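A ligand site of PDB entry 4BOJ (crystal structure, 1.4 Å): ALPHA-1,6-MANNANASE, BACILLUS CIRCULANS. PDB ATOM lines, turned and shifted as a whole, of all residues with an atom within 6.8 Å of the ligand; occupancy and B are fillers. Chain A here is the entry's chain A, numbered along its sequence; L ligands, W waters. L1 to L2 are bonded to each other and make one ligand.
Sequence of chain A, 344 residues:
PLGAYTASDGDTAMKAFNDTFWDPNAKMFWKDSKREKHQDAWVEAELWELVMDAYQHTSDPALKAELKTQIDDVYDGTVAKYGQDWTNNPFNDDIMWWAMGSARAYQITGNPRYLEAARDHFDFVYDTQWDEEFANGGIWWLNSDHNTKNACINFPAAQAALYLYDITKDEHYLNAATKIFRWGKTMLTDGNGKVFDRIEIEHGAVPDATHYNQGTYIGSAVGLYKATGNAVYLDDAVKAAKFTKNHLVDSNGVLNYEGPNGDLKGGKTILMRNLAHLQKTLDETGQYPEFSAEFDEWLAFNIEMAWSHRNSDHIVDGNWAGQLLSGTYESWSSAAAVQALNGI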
ATOM      1  N   TRP A  42      28.249 -24.046 -13.530  1.00  0.00           N
ATOM      2  CA  TRP A  42      27.480 -24.681 -12.434  1.00  0.00           C
ATOM      3  C   TRP A  42      27.902 -26.118 -12.242  1.00  0.00           C
ATOM      4  O   TRP A  42      27.992 -26.625 -11.123  1.00  0.00           O
ATOM      5  CB  TRP A  42      25.945 -24.553 -12.617  1.00  0.00           C
ATOM      6  CG  TRP A  42      25.264 -25.612 -13.427  1.00  0.00           C
ATOM      7  CD1 TRP A  42      24.997 -25.574 -14.778  1.00  0.00           C
ATOM      8  CD2 TRP A  42      24.694 -26.825 -12.940  1.00  0.00           C
ATOM      9  NE1 TRP A  42      24.303 -26.712 -15.155  1.00  0.00           N
ATOM     10  CE2 TRP A  42      24.100 -27.502 -14.042  1.00  0.00           C
ATOM     11  CE3 TRP A  42      24.609 -27.398 -11.662  1.00  0.00           C
ATOM     12  CZ2 TRP A  42      23.466 -28.747 -13.901  1.00  0.00           C
ATOM     13  CZ3 TRP A  42      23.973 -28.601 -11.517  1.00  0.00           C
ATOM     14  CH2 TRP A  42      23.400 -29.269 -12.627  1.00  0.00           C
ATOM     15  N   ASP A  93      20.570 -20.120  -9.785  1.00  0.00           N
ATOM     16  CA  ASP A  93      21.070 -21.464  -9.495  1.00  0.00           C
ATOM     17  C   ASP A  93      22.603 -21.564  -9.589  1.00  0.00           C
ATOM     18  O   ASP A  93      23.197 -22.154  -8.689  1.00  0.00           O
ATOM     19  CB  ASP A  93      20.311 -22.549 -10.291  1.00  0.00           C
ATOM     20  CG  ASP A  93      20.329 -22.355 -11.789  1.00  0.00           C
ATOM     21  OD1 ASP A  93      20.717 -21.277 -12.298  1.00  0.00           O
ATOM     22  OD2 ASP A  93      19.874 -23.311 -12.460  1.00  0.00           O
ATOM     23  N   TRP A 141      14.349 -18.486 -10.477  1.00  0.00           N
ATOM     24  CA  TRP A 141      15.437 -19.156 -11.189  1.00  0.00           C
ATOM     25  C   TRP A 141      16.509 -18.140 -11.616  1.00  0.00           C
ATOM     26  O   TRP A 141      17.711 -18.401 -11.461  1.00  0.00           O
ATOM     27  CB  TRP A 141      14.876 -19.867 -12.425  1.00  0.00           C
ATOM     28  CG  TRP A 141      15.867 -20.675 -13.153  1.00  0.00           C
ATOM     29  CD1 TRP A 141      16.801 -21.518 -12.626  1.00  0.00           C
ATOM     30  CD2 TRP A 141      16.019 -20.754 -14.558  1.00  0.00           C
ATOM     31  NE1 TRP A 141      17.540 -22.118 -13.620  1.00  0.00           N
ATOM     32  CE2 TRP A 141      17.070 -21.655 -14.831  1.00  0.00           C
ATOM     33  CE3 TRP A 141      15.329 -20.172 -15.641  1.00  0.00           C
ATOM     34  CZ2 TRP A 141      17.472 -21.997 -16.128  1.00  0.00           C
ATOM     35  CZ3 TRP A 141      15.739 -20.485 -16.945  1.00  0.00           C
ATOM     36  CH2 TRP A 141      16.810 -21.389 -17.165  1.00  0.00           C
ATOM     37  N   THR A 148       9.980 -17.798 -13.469  1.00  0.00           N
ATOM     38  CA  THR A 148       9.831 -19.198 -12.980  1.00  0.00           C
ATOM     39  C   THR A 148      10.542 -19.397 -11.669  1.00  0.00           C
ATOM     40  O   THR A 148      11.511 -18.697 -11.410  1.00  0.00           O
ATOM     41  CB  THR A 148      10.353 -20.270 -13.970  1.00  0.00           C
ATOM     42  OG1 THR A 148      11.774 -20.205 -14.125  1.00  0.00           O
ATOM     43  CG2 THR A 148       9.762 -20.151 -15.349  1.00  0.00           C
ATOM     44  N   ASN A 150      12.136 -22.583  -9.418  1.00  0.00           N
ATOM     45  CA  ASN A 150      12.545 -23.919  -9.816  1.00  0.00           C
ATOM     46  C   ASN A 150      13.095 -24.751  -8.654  1.00  0.00           C
ATOM     47  O   ASN A 150      13.733 -24.195  -7.737  1.00  0.00           O
ATOM     48  CB  ASN A 150      13.625 -23.860 -10.907  1.00  0.00           C
ATOM     49  CG  ASN A 150      13.176 -23.148 -12.178  1.00  0.00           C
ATOM     50  OD1 ASN A 150      12.440 -22.175 -12.141  1.00  0.00           O
ATOM     51  ND2 ASN A 150      13.652 -23.691 -13.292  1.00  0.00           N
ATOM     52  N   ALA A 151      12.919 -26.061  -8.722  1.00  0.00           N
ATOM     53  CA  ALA A 151      13.533 -26.943  -7.735  1.00  0.00           C
ATOM     54  C   ALA A 151      15.041 -26.765  -7.709  1.00  0.00           C
ATOM     55  O   ALA A 151      15.652 -26.845  -6.633  1.00  0.00           O
ATOM     56  CB  ALA A 151      13.161 -28.394  -8.044  1.00  0.00           C
ATOM     57  N   CYS A 152      15.661 -26.535  -8.864  1.00  0.00           N
ATOM     58  CA  CYS A 152      17.123 -26.510  -8.962  1.00  0.00           C
ATOM     59  C   CYS A 152      17.773 -25.280  -8.387  1.00  0.00           C
ATOM     60  O   CYS A 152      18.982 -25.259  -8.337  1.00  0.00           O
ATOM     61  CB  CYS A 152      17.570 -26.700 -10.414  1.00  0.00           C
ATOM     62  SG  CYS A 152      17.073 -25.295 -11.518  1.00  0.00           S
ATOM     63  N   ILE A 153      16.976 -24.286  -8.009  1.00  0.00           N
ATOM     64  CA  ILE A 153      17.491 -23.207  -7.123  1.00  0.00           C
ATOM     65  C   ILE A 153      16.987 -23.415  -5.699  1.00  0.00           C
ATOM     66  O   ILE A 153      17.743 -23.257  -4.738  1.00  0.00           O
ATOM     67  CB  ILE A 153      17.203 -21.743  -7.663  1.00  0.00           C
ATOM     68  CG1 ILE A 153      17.544 -20.668  -6.598  1.00  0.00           C
ATOM     69  CG2 ILE A 153      15.743 -21.579  -8.168  1.00  0.00           C
ATOM     70  CD1 ILE A 153      18.942 -20.649  -6.166  1.00  0.00           C
ATOM     71  N   ASP A 197       9.765 -29.948 -11.512  1.00  0.00           N
ATOM     72  CA  ASP A 197      10.866 -29.138 -11.999  1.00  0.00           C
ATOM     73  C   ASP A 197      10.717 -27.686 -11.580  1.00  0.00           C
ATOM     74  O   ASP A 197      11.708 -27.059 -11.146  1.00  0.00           O
ATOM     75  CB  ASP A 197      10.974 -29.231 -13.508  1.00  0.00           C
ATOM     76  CG  ASP A 197      12.298 -28.726 -13.980  1.00  0.00           C
ATOM     77  OD1 ASP A 197      13.272 -29.527 -13.858  1.00  0.00           O
ATOM     78  OD2 ASP A 197      12.365 -27.540 -14.428  1.00  0.00           O
ATOM     79  N   ARG A 198       9.544 -27.085 -11.785  1.00  0.00           N
ATOM     80  CA  ARG A 198       9.382 -25.698 -11.572  1.00  0.00           C
ATOM     81  C   ARG A 198       7.922 -25.270 -11.659  1.00  0.00           C
ATOM     82  O   ARG A 198       7.073 -26.081 -12.038  1.00  0.00           O
ATOM     83  CB  ARG A 198      10.213 -24.895 -12.610  1.00  0.00           C
ATOM     84  CG  ARG A 198       9.717 -25.083 -14.072  1.00  0.00           C
ATOM     85  CD  ARG A 198      10.758 -24.564 -15.095  1.00  0.00           C
ATOM     86  NE  ARG A 198      10.190 -24.688 -16.451  1.00  0.00           N
ATOM     87  CZ  ARG A 198      10.210 -25.820 -17.138  1.00  0.00           C
ATOM     88  NH1 ARG A 198      10.748 -26.950 -16.695  1.00  0.00           N
ATOM     89  NH2 ARG A 198       9.608 -25.849 -18.323  1.00  0.00           N
ATOM     90  N   GLU A 200       5.862 -21.945 -13.391  1.00  0.00           N
ATOM     91  CA  GLU A 200       6.025 -20.809 -14.285  1.00  0.00           C
ATOM     92  C   GLU A 200       4.883 -19.830 -14.134  1.00  0.00           C
ATOM     93  O   GLU A 200       3.737 -20.240 -14.028  1.00  0.00           O
ATOM     94  CB  GLU A 200       6.116 -21.279 -15.730  1.00  0.00           C
ATOM     95  CG  GLU A 200       7.169 -22.313 -16.011  1.00  0.00           C
ATOM     96  CD  GLU A 200       7.814 -22.091 -17.369  1.00  0.00           C
ATOM     97  OE1 GLU A 200       7.431 -21.088 -18.035  1.00  0.00           O
ATOM     98  OE2 GLU A 200       8.720 -22.849 -17.773  1.00  0.00           O
ATOM     99  N   VAL A 206       5.160 -27.425 -13.743  1.00  0.00           N
ATOM    100  CA  VAL A 206       5.726 -28.351 -14.685  1.00  0.00           C
ATOM    101  C   VAL A 206       6.199 -29.557 -13.871  1.00  0.00           C
ATOM    102  O   VAL A 206       7.329 -29.527 -13.319  1.00  0.00           O
ATOM    103  CB  VAL A 206       6.885 -27.703 -15.453  1.00  0.00           C
ATOM    104  CG1 VAL A 206       7.431 -28.686 -16.467  1.00  0.00           C
ATOM    105  CG2 VAL A 206       6.418 -26.404 -16.129  1.00  0.00           C
ATOM    106  N   ASP A 208       7.603 -32.439 -14.019  1.00  0.00           N
ATOM    107  CA  ASP A 208       8.567 -33.338 -14.625  1.00  0.00           C
ATOM    108  C   ASP A 208       9.626 -33.555 -13.545  1.00  0.00           C
ATOM    109  O   ASP A 208      10.259 -32.560 -13.118  1.00  0.00           O
ATOM    110  CB  ASP A 208       9.329 -32.659 -15.805  1.00  0.00           C
ATOM    111  CG  ASP A 208       8.539 -32.472 -17.099  1.00  0.00           C
ATOM    112  OD1 ASP A 208       7.547 -33.169 -17.331  1.00  0.00           O
ATOM    113  OD2 ASP A 208       8.955 -31.581 -17.917  1.00  0.00           O
ATOM    114  N   ALA A 209       9.835 -34.795 -13.151  1.00  0.00           N
ATOM    115  CA  ALA A 209      10.828 -35.124 -12.123  1.00  0.00           C
ATOM    116  C   ALA A 209      12.130 -35.595 -12.739  1.00  0.00           C
ATOM    117  O   ALA A 209      12.154 -36.250 -13.784  1.00  0.00           O
ATOM    118  CB  ALA A 209      10.263 -36.217 -11.199  1.00  0.00           C
ATOM    119  N   THR A 210      13.239 -35.294 -12.056  1.00  0.00           N
ATOM    120  CA  THR A 210      14.577 -35.672 -12.508  1.00  0.00           C
ATOM    121  C   THR A 210      15.453 -36.035 -11.342  1.00  0.00           C
ATOM    122  O   THR A 210      15.155 -35.682 -10.170  1.00  0.00           O
ATOM    123  CB  THR A 210      15.275 -34.518 -13.277  1.00  0.00           C
ATOM    124  OG1 THR A 210      15.328 -33.376 -12.443  1.00  0.00           O
ATOM    125  CG2 THR A 210      14.518 -34.178 -14.588  1.00  0.00           C
ATOM    126  N   TYR A 212      18.435 -34.968 -10.292  1.00  0.00           N
ATOM    127  CA  TYR A 212      19.115 -34.001  -9.421  1.00  0.00           C
ATOM    128  C   TYR A 212      18.148 -33.275  -8.508  1.00  0.00           C
ATOM    129  O   TYR A 212      18.543 -32.825  -7.428  1.00  0.00           O
ATOM    130  CB  TYR A 212      20.031 -33.023 -10.179  1.00  0.00           C
ATOM    131  CG  TYR A 212      19.377 -31.872 -10.949  1.00  0.00           C
ATOM    132  CD1 TYR A 212      18.216 -32.032 -11.721  1.00  0.00           C
ATOM    133  CD2 TYR A 212      19.991 -30.613 -10.956  1.00  0.00           C
ATOM    134  CE1 TYR A 212      17.696 -30.943 -12.452  1.00  0.00           C
ATOM    135  CE2 TYR A 212      19.469 -29.545 -11.702  1.00  0.00           C
ATOM    136  CZ  TYR A 212      18.322 -29.736 -12.429  1.00  0.00           C
ATOM    137  OH  TYR A 212      17.872 -28.637 -13.165  1.00  0.00           O
ATOM    138  N   ASN A 213      16.905 -33.119  -8.915  1.00  0.00           N
ATOM    139  CA  ASN A 213      15.921 -32.459  -8.063  1.00  0.00           C
ATOM    140  C   ASN A 213      15.413 -33.437  -6.982  1.00  0.00           C
ATOM    141  O   ASN A 213      15.204 -32.992  -5.834  1.00  0.00           O
ATOM    142  CB  ASN A 213      14.783 -31.865  -8.888  1.00  0.00           C
ATOM    143  CG  ASN A 213      15.209 -30.587  -9.589  1.00  0.00           C
ATOM    144  OD1 ASN A 213      16.042 -29.817  -9.100  1.00  0.00           O
ATOM    145  ND2 ASN A 213      14.562 -30.289 -10.721  1.00  0.00           N
ATOM    146  N   ASN A 261      19.708 -33.741 -22.786  1.00  0.00           N
ATOM    147  CA  ASN A 261      19.815 -32.459 -22.120  1.00  0.00           C
ATOM    148  C   ASN A 261      21.150 -32.378 -21.343  1.00  0.00           C
ATOM    149  O   ASN A 261      21.435 -33.273 -20.522  1.00  0.00           O
ATOM    150  CB  ASN A 261      18.637 -32.256 -21.196  1.00  0.00           C
ATOM    151  CG  ASN A 261      18.691 -30.953 -20.480  1.00  0.00           C
ATOM    152  OD1 ASN A 261      19.475 -30.784 -19.475  1.00  0.00           O
ATOM    153  ND2 ASN A 261      17.860 -29.985 -20.922  1.00  0.00           N
ATOM    154  N   ASP A 263      22.378 -30.424 -19.005  1.00  0.00           N
ATOM    155  CA  ASP A 263      22.296 -30.255 -17.538  1.00  0.00           C
ATOM    156  C   ASP A 263      21.912 -31.544 -16.841  1.00  0.00           C
ATOM    157  O   ASP A 263      22.424 -31.858 -15.750  1.00  0.00           O
ATOM    158  CB  ASP A 263      21.313 -29.161 -17.182  1.00  0.00           C
ATOM    159  CG  ASP A 263      21.733 -27.826 -17.749  1.00  0.00           C
ATOM    160  OD1 ASP A 263      22.940 -27.500 -17.620  1.00  0.00           O
ATOM    161  OD2 ASP A 263      20.890 -27.182 -18.442  1.00  0.00           O
ATOM    162  N   LEU A 264      21.046 -32.338 -17.463  1.00  0.00           N
ATOM    163  CA  LEU A 264      20.551 -33.569 -16.832  1.00  0.00           C
ATOM    164  C   LEU A 264      21.456 -34.772 -16.991  1.00  0.00           C
ATOM    165  O   LEU A 264      21.350 -35.711 -16.189  1.00  0.00           O
ATOM    166  CB  LEU A 264      19.167 -33.930 -17.392  1.00  0.00           C
ATOM    167  CG  LEU A 264      18.033 -32.919 -17.202  1.00  0.00           C
ATOM    168  CD1 LEU A 264      16.741 -33.485 -17.741  1.00  0.00           C
ATOM    169  CD2 LEU A 264      17.885 -32.555 -15.726  1.00  0.00           C
HETATM  170  C1  LIG L   1      16.918 -25.555 -16.786  1.00  0.00           C
HETATM  171  C2  LIG L   1      15.779 -25.322 -15.797  1.00  0.00           C
HETATM  172  C3  LIG L   1      15.827 -26.476 -14.831  1.00  0.00           C
HETATM  173  C4  LIG L   1      15.636 -27.772 -15.615  1.00  0.00           C
HETATM  174  C5  LIG L   1      16.720 -27.962 -16.644  1.00  0.00           C
HETATM  175  C6  LIG L   1      16.545 -29.199 -17.508  1.00  0.00           C
HETATM  176  O1  LIG L   1      18.196 -25.471 -16.205  1.00  0.00           O
HETATM  177  O2  LIG L   1      14.531 -25.204 -16.466  1.00  0.00           O
HETATM  178  O3  LIG L   1      14.720 -26.321 -13.900  1.00  0.00           O
HETATM  179  O4  LIG L   1      15.684 -28.932 -14.742  1.00  0.00           O
HETATM  180  O5  LIG L   1      16.753 -26.814 -17.506  1.00  0.00           O
HETATM  181  O6  LIG L   1      15.315 -29.007 -18.336  1.00  0.00           O
HETATM  182  C1  LG2 L   2      14.997 -30.190 -19.026  1.00  0.00           C
HETATM  183  C2  LG2 L   2      14.020 -29.818 -20.118  1.00  0.00           C
HETATM  184  C3  LG2 L   2      12.683 -29.308 -19.489  1.00  0.00           C
HETATM  185  C4  LG2 L   2      12.080 -30.304 -18.546  1.00  0.00           C
HETATM  186  C5  LG2 L   2      13.120 -30.555 -17.430  1.00  0.00           C
HETATM  187  C6  LG2 L   2      12.611 -31.583 -16.413  1.00  0.00           C
HETATM  188  O1  LG2 L   2      13.731 -30.992 -20.810  1.00  0.00           O
HETATM  189  O2  LG2 L   2      11.644 -29.113 -20.546  1.00  0.00           O
HETATM  190  O3  LG2 L   2      10.932 -29.660 -17.888  1.00  0.00           O
HETATM  191  O4  LG2 L   2      14.314 -31.062 -18.012  1.00  0.00           O
HETATM  192  O5  LG2 L   2      12.343 -32.834 -17.041  1.00  0.00           O
HETATM  193  O   HOH W   1      19.906 -27.150 -14.382  1.00  0.00           O
HETATM  194  O   HOH W   2       9.406 -27.798 -20.329  1.00  0.00           O
HETATM  195  O   HOH W   3      14.129 -26.363 -18.836  1.00  0.00           O
HETATM  196  O   HOH W   4      11.507 -35.347 -16.326  1.00  0.00           O
HETATM  197  O   HOH W   5      19.499 -24.291 -18.309  1.00  0.00           O
HETATM  198  O   HOH W   6      14.422 -27.393 -11.357  1.00  0.00           O
HETATM  199  O   HOH W   7      13.535 -22.706 -16.139  1.00  0.00           O
HETATM  200  O   HOH W   8      12.873 -33.025 -23.331  1.00  0.00           O
HETATM  201  O   HOH W   9      18.363 -27.305 -19.759  1.00  0.00           O
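OD1 of Asp 197 lies within hydrogen-bond range of O4 of LIG L1 (2.6 Å).
An oxygen (O4) of LIG L1 lies within hydrogen-bond range of the side-chain hydroxyl (OH) of Tyr 212 (2.7 Å).
The side-chain carboxylate of Asp 208 lies within hydrogen-bond range of an oxygen (O3) of LG2 L2, 2.8 Å away.
An oxygen (O3) of LIG L1 sits at hydrogen-bond distance from the side-chain amide nitrogen (ND2) of Asn 150, at 2.9 Å.
An oxygen (O3) of LG2 L2 sits at hydrogen-bond distance from the guanidinium group (NH1) of Arg 198 (3.0 Å).
An oxygen (O3) of LIG L1 lies within hydrogen-bond range of the side-chain sulfur of Cys 152, 3.5 Å away.
The backbone NH (N) of Asp 197 lies within hydrogen-bond range of the backbone carbonyl oxygen (O) of Asp 208.
The backbone carbonyl oxygen of Asp 197 is in hydrogen-bond range of the backbone NH of Ala 151, at 2.9 Å.
NE of Arg 198 lies within salt-bridge range of OE2 of Glu 200 (2.7 Å).
The side-chain amide oxygen (OD1) of Asn 261 lies within hydrogen-bond range of the backbone NH (N) of Leu 264 (3.0 Å).
N of Asp 263 lies within hydrogen-bond range of OD1 of Asn 261, at 3.0 Å.
The backbone NH of Cys 152 sits at hydrogen-bond distance from the side-chain amide oxygen of Asn 213.
The backbone carbonyl oxygen (O) of Thr 148 is in hydrogen-bond range of the backbone NH (N) of Trp 141 (3.0 Å).
The side-chain carboxylate (OD1) of Asp 263 lies within hydrogen-bond range of the indole nitrogen (NE1) of Trp 42 (2.9 Å).
Merely in contact with the ligand: Asn 261 (3.4 Å), Leu 264 (3.4 Å), Thr 210 (3.5 Å), Trp 141 (3.5 Å), Asp 263 (3.9 Å) and Val 206 (3.9 Å).
The nearest printed residue that does not touch the ligand is Asn 213 (4.4 Å).
Water W2 lies within hydrogen-bond range of O2 of LG2 L2 (2.6 Å) and NH2 of Arg 198 (2.8 Å).
Water W7 lies within hydrogen-bond range of an oxygen (O2) of LIG L1 and the side-chain amide nitrogen of Asn 150.
Water W5 bridges O1 of LIG L1 (2.7 Å) and OD2 of Asp 263 (3.2 Å).
Water W4 bridges an oxygen (O5) of LG2 L2 (2.7 Å) and the backbone carbonyl oxygen of Ala 209 (2.8 Å).
Water W9 lies within hydrogen-bond range of O5 of LIG L1 (2.8 Å), OD2 of Asp 263 (2.9 Å) and ND2 of Asn 261 (3.0 Å).
Water W1 bridges OH of Tyr 212 and O1 of LIG L1.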
